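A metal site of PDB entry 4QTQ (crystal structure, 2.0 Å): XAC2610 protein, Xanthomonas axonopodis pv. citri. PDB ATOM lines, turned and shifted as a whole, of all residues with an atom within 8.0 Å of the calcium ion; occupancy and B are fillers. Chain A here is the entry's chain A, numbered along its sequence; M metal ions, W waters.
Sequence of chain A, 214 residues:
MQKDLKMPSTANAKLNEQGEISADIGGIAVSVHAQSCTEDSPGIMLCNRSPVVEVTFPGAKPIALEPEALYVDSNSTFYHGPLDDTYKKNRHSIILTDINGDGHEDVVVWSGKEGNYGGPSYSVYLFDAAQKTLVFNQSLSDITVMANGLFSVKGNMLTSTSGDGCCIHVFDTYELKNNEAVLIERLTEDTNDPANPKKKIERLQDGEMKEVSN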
ATOM      1  N   THR A  97       7.598 -26.022 -32.049  1.00  0.00           N
ATOM      2  CA  THR A  97       6.742 -24.975 -31.527  1.00  0.00           C
ATOM      3  C   THR A  97       7.386 -24.453 -30.244  1.00  0.00           C
ATOM      4  O   THR A  97       7.948 -25.236 -29.471  1.00  0.00           O
ATOM      5  CB  THR A  97       5.323 -25.506 -31.231  1.00  0.00           C
ATOM      6  OG1 THR A  97       4.447 -24.421 -30.924  1.00  0.00           O
ATOM      7  CG2 THR A  97       5.315 -26.499 -30.053  1.00  0.00           C
ATOM      8  N   ASP A  98       7.329 -23.142 -30.027  1.00  0.00           N
ATOM      9  CA  ASP A  98       7.902 -22.537 -28.835  1.00  0.00           C
ATOM     10  C   ASP A  98       6.840 -22.566 -27.774  1.00  0.00           C
ATOM     11  O   ASP A  98       5.874 -21.828 -27.841  1.00  0.00           O
ATOM     12  CB  ASP A  98       8.354 -21.087 -29.082  1.00  0.00           C
ATOM     13  CG  ASP A  98       9.021 -20.444 -27.872  1.00  0.00           C
ATOM     14  OD1 ASP A  98       9.545 -21.177 -26.981  1.00  0.00           O
ATOM     15  OD2 ASP A  98       9.027 -19.192 -27.819  1.00  0.00           O
ATOM     16  N   ILE A  99       7.012 -23.445 -26.801  1.00  0.00           N
ATOM     17  CA  ILE A  99       6.002 -23.664 -25.780  1.00  0.00           C
ATOM     18  C   ILE A  99       6.163 -22.623 -24.673  1.00  0.00           C
ATOM     19  O   ILE A  99       5.178 -22.079 -24.183  1.00  0.00           O
ATOM     20  CB  ILE A  99       6.073 -25.102 -25.214  1.00  0.00           C
ATOM     21  CG1 ILE A  99       5.686 -26.095 -26.326  1.00  0.00           C
ATOM     22  CG2 ILE A  99       5.159 -25.268 -24.009  1.00  0.00           C
ATOM     23  CD1 ILE A  99       5.901 -27.557 -25.985  1.00  0.00           C
ATOM     24  N   ASN A 100       7.413 -22.328 -24.303  1.00  0.00           N
ATOM     25  CA  ASN A 100       7.660 -21.455 -23.160  1.00  0.00           C
ATOM     26  C   ASN A 100       7.933 -19.973 -23.492  1.00  0.00           C
ATOM     27  O   ASN A 100       8.320 -19.207 -22.619  1.00  0.00           O
ATOM     28  CB  ASN A 100       8.772 -22.023 -22.260  1.00  0.00           C
ATOM     29  CG  ASN A 100      10.096 -22.172 -22.973  1.00  0.00           C
ATOM     30  OD1 ASN A 100      10.218 -22.012 -24.188  1.00  0.00           O
ATOM     31  ND2 ASN A 100      11.108 -22.518 -22.202  1.00  0.00           N
ATOM     32  N   GLY A 101       7.703 -19.584 -24.745  1.00  0.00           N
ATOM     33  CA  GLY A 101       7.721 -18.176 -25.144  1.00  0.00           C
ATOM     34  C   GLY A 101       9.056 -17.453 -25.127  1.00  0.00           C
ATOM     35  O   GLY A 101       9.098 -16.225 -25.149  1.00  0.00           O
ATOM     36  N   ASP A 102      10.160 -18.198 -25.121  1.00  0.00           N
ATOM     37  CA  ASP A 102      11.482 -17.573 -25.093  1.00  0.00           C
ATOM     38  C   ASP A 102      12.082 -17.321 -26.477  1.00  0.00           C
ATOM     39  O   ASP A 102      13.231 -16.907 -26.580  1.00  0.00           O
ATOM     40  CB  ASP A 102      12.444 -18.407 -24.231  1.00  0.00           C
ATOM     41  CG  ASP A 102      12.834 -19.743 -24.892  1.00  0.00           C
ATOM     42  OD1 ASP A 102      12.223 -20.150 -25.899  1.00  0.00           O
ATOM     43  OD2 ASP A 102      13.769 -20.385 -24.379  1.00  0.00           O
ATOM     44  N   GLY A 103      11.332 -17.589 -27.534  1.00  0.00           N
ATOM     45  CA  GLY A 103      11.802 -17.301 -28.896  1.00  0.00           C
ATOM     46  C   GLY A 103      12.554 -18.437 -29.582  1.00  0.00           C
ATOM     47  O   GLY A 103      12.951 -18.297 -30.735  1.00  0.00           O
ATOM     48  N   HIS A 104      12.750 -19.552 -28.881  1.00  0.00           N
ATOM     49  CA  HIS A 104      13.355 -20.738 -29.492  1.00  0.00           C
ATOM     50  C   HIS A 104      12.401 -21.920 -29.515  1.00  0.00           C
ATOM     51  O   HIS A 104      11.793 -22.251 -28.497  1.00  0.00           O
ATOM     52  CB  HIS A 104      14.629 -21.149 -28.770  1.00  0.00           C
ATOM     53  CG  HIS A 104      15.505 -22.010 -29.606  1.00  0.00           C
ATOM     54  ND1 HIS A 104      15.293 -23.369 -29.749  1.00  0.00           N
ATOM     55  CD2 HIS A 104      16.550 -21.709 -30.415  1.00  0.00           C
ATOM     56  CE1 HIS A 104      16.200 -23.871 -30.568  1.00  0.00           C
ATOM     57  NE2 HIS A 104      16.970 -22.881 -30.985  1.00  0.00           N
ATOM     58  N   GLU A 105      12.294 -22.574 -30.673  1.00  0.00           N
ATOM     59  CA  GLU A 105      11.371 -23.678 -30.797  1.00  0.00           C
ATOM     60  C   GLU A 105      11.781 -24.826 -29.885  1.00  0.00           C
ATOM     61  O   GLU A 105      12.970 -25.089 -29.662  1.00  0.00           O
ATOM     62  CB  GLU A 105      11.261 -24.210 -32.223  1.00  0.00           C
ATOM     63  CG  GLU A 105      10.385 -23.391 -33.140  1.00  0.00           C
ATOM     64  CD  GLU A 105      11.177 -22.364 -33.880  1.00  0.00           C
ATOM     65  OE1 GLU A 105      12.271 -21.984 -33.385  1.00  0.00           O
ATOM     66  OE2 GLU A 105      10.718 -21.939 -34.961  1.00  0.00           O
ATOM     67  N   ASP A 106      10.755 -25.469 -29.344  1.00  0.00           N
ATOM     68  CA  ASP A 106      10.862 -26.675 -28.584  1.00  0.00           C
ATOM     69  C   ASP A 106      10.296 -27.805 -29.442  1.00  0.00           C
ATOM     70  O   ASP A 106       9.848 -27.579 -30.568  1.00  0.00           O
ATOM     71  CB  ASP A 106      10.072 -26.495 -27.294  1.00  0.00           C
ATOM     72  CG  ASP A 106      10.430 -25.208 -26.572  1.00  0.00           C
ATOM     73  OD1 ASP A 106      11.631 -25.027 -26.246  1.00  0.00           O
ATOM     74  OD2 ASP A 106       9.535 -24.360 -26.357  1.00  0.00           O
ATOM     75  N   VAL A 107      10.318 -29.029 -28.928  1.00  0.00           N
ATOM     76  CA  VAL A 107       9.946 -30.183 -29.735  1.00  0.00           C
ATOM     77  C   VAL A 107       8.965 -31.081 -28.979  1.00  0.00           C
ATOM     78  O   VAL A 107       9.125 -31.340 -27.768  1.00  0.00           O
ATOM     79  CB  VAL A 107      11.188 -30.987 -30.184  1.00  0.00           C
ATOM     80  CG1 VAL A 107      10.783 -32.193 -31.025  1.00  0.00           C
ATOM     81  CG2 VAL A 107      12.140 -30.092 -30.951  1.00  0.00           C
ATOM     82  N   TYR A 125       9.983 -31.763 -25.172  1.00  0.00           N
ATOM     83  CA  TYR A 125      11.368 -31.344 -24.948  1.00  0.00           C
ATOM     84  C   TYR A 125      11.527 -29.832 -25.143  1.00  0.00           C
ATOM     85  O   TYR A 125      11.287 -29.297 -26.245  1.00  0.00           O
ATOM     86  CB  TYR A 125      12.326 -32.061 -25.907  1.00  0.00           C
ATOM     87  CG  TYR A 125      12.168 -33.572 -25.976  1.00  0.00           C
ATOM     88  CD1 TYR A 125      11.103 -34.142 -26.663  1.00  0.00           C
ATOM     89  CD2 TYR A 125      13.076 -34.427 -25.369  1.00  0.00           C
ATOM     90  CE1 TYR A 125      10.933 -35.516 -26.737  1.00  0.00           C
ATOM     91  CE2 TYR A 125      12.922 -35.811 -25.421  1.00  0.00           C
ATOM     92  CZ  TYR A 125      11.841 -36.350 -26.109  1.00  0.00           C
ATOM     93  OH  TYR A 125      11.657 -37.693 -26.213  1.00  0.00           O
ATOM     94  N   LEU A 126      11.925 -29.131 -24.085  1.00  0.00           N
ATOM     95  CA  LEU A 126      12.192 -27.699 -24.162  1.00  0.00           C
ATOM     96  C   LEU A 126      13.665 -27.443 -24.514  1.00  0.00           C
ATOM     97  O   LEU A 126      14.567 -28.082 -23.976  1.00  0.00           O
ATOM     98  CB  LEU A 126      11.847 -27.003 -22.837  1.00  0.00           C
ATOM     99  CG  LEU A 126      10.387 -27.050 -22.380  1.00  0.00           C
ATOM    100  CD1 LEU A 126      10.237 -26.233 -21.115  1.00  0.00           C
ATOM    101  CD2 LEU A 126       9.444 -26.525 -23.459  1.00  0.00           C
ATOM    102  N   PHE A 127      13.897 -26.494 -25.402  1.00  0.00           N
ATOM    103  CA  PHE A 127      15.248 -26.091 -25.688  1.00  0.00           C
ATOM    104  C   PHE A 127      15.804 -25.356 -24.468  1.00  0.00           C
ATOM    105  O   PHE A 127      15.216 -24.397 -23.986  1.00  0.00           O
ATOM    106  CB  PHE A 127      15.324 -25.176 -26.915  1.00  0.00           C
ATOM    107  CG  PHE A 127      16.717 -24.922 -27.363  1.00  0.00           C
ATOM    108  CD1 PHE A 127      17.439 -25.920 -28.000  1.00  0.00           C
ATOM    109  CD2 PHE A 127      17.317 -23.697 -27.133  1.00  0.00           C
ATOM    110  CE1 PHE A 127      18.743 -25.692 -28.408  1.00  0.00           C
ATOM    111  CE2 PHE A 127      18.623 -23.462 -27.548  1.00  0.00           C
ATOM    112  CZ  PHE A 127      19.326 -24.458 -28.187  1.00  0.00           C
ATOM    113  N   ASP A 128      16.919 -25.856 -23.951  1.00  0.00           N
ATOM    114  CA  ASP A 128      17.556 -25.257 -22.795  1.00  0.00           C
ATOM    115  C   ASP A 128      18.706 -24.416 -23.317  1.00  0.00           C
ATOM    116  O   ASP A 128      19.725 -24.944 -23.739  1.00  0.00           O
ATOM    117  CB  ASP A 128      18.048 -26.359 -21.844  1.00  0.00           C
ATOM    118  CG  ASP A 128      18.356 -25.829 -20.458  1.00  0.00           C
ATOM    119  OD1 ASP A 128      19.229 -24.954 -20.323  1.00  0.00           O
ATOM    120  OD2 ASP A 128      17.707 -26.303 -19.498  1.00  0.00           O
ATOM    121  N   ALA A 129      18.500 -23.102 -23.297  1.00  0.00           N
ATOM    122  CA  ALA A 129      19.438 -22.134 -23.871  1.00  0.00           C
ATOM    123  C   ALA A 129      20.862 -22.216 -23.295  1.00  0.00           C
ATOM    124  O   ALA A 129      21.838 -21.968 -24.000  1.00  0.00           O
ATOM    125  CB  ALA A 129      18.892 -20.720 -23.697  1.00  0.00           C
ATOM    126  N   LEU A 134      18.028 -29.939 -26.015  1.00  0.00           N
ATOM    127  CA  LEU A 134      16.610 -30.133 -25.805  1.00  0.00           C
ATOM    128  C   LEU A 134      16.508 -31.050 -24.616  1.00  0.00           C
ATOM    129  O   LEU A 134      17.131 -32.094 -24.618  1.00  0.00           O
ATOM    130  CB  LEU A 134      15.978 -30.772 -27.047  1.00  0.00           C
ATOM    131  CG  LEU A 134      15.768 -29.797 -28.208  1.00  0.00           C
ATOM    132  CD1 LEU A 134      15.789 -30.503 -29.551  1.00  0.00           C
ATOM    133  CD2 LEU A 134      14.466 -29.042 -27.988  1.00  0.00           C
ATOM    134  N   LEU A 176       2.926 -21.775 -16.997  1.00  0.00           N
ATOM    135  CA  LEU A 176       4.282 -22.251 -17.206  1.00  0.00           C
ATOM    136  C   LEU A 176       5.244 -21.153 -16.814  1.00  0.00           C
ATOM    137  O   LEU A 176       5.225 -20.077 -17.423  1.00  0.00           O
ATOM    138  CB  LEU A 176       4.506 -22.644 -18.654  1.00  0.00           C
ATOM    139  CG  LEU A 176       5.901 -23.265 -18.918  1.00  0.00           C
ATOM    140  CD1 LEU A 176       5.955 -24.731 -18.504  1.00  0.00           C
ATOM    141  CD2 LEU A 176       6.264 -23.111 -20.374  1.00  0.00           C
HETATM  142 CA    CA M   1      11.332 -22.471 -26.192  1.00  0.00          CA
HETATM  143  O   HOH W   1      13.298 -22.879 -25.058  1.00  0.00           O
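The backbone NH (N) of Asp 106 is in hydrogen-bond range of the backbone carbonyl oxygen (O) of Thr 97, at 2.8 Å.
The backbone NH (N) of Ile 99 lies close to the side-chain carboxylate (OD2) of Asp 106 (2.7 Å).
The side-chain carboxylate (OD2) of Asp 98 sits at hydrogen-bond distance from the backbone NH (N) of Gly 103 (2.8 Å).
OD1 of Asp 106 lies close to N of Phe 127, 2.8 Å away.
The side-chain carboxylate (OD2) of Asp 98 sits close to the backbone NH (N) of Gly 101 (3.4 Å).
Within 4 Å of the calcium ion: Asp 98, Asn 100, Asp 102, His 104 and Asp 106.
Along chain A the residues within 4 Å of the calcium ion span positions 98 to 106.
The calcium ion is bound by water W1 (2.3 Å).
The side-chain amide oxygen (OD1) of Asn 100 binds the calcium ion, 2.3 Å away.
OD1 of Asp 98 is bound to the calcium ion, 2.3 Å away.
O of His 104 binds the calcium ion (2.4 Å).
The side-chain carboxylate (OD1) of Asp 102 binds the calcium ion.
OD1 of Asp 106 binds the calcium ion (2.6 Å).
The calcium ion is bound by the side-chain carboxylate (OD2) of Asp 106 (2.6 Å).
The calcium ion has seven donor atoms within binding distance.
Water W1 bridges OD2 of Asp 102 and O of Phe 127.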
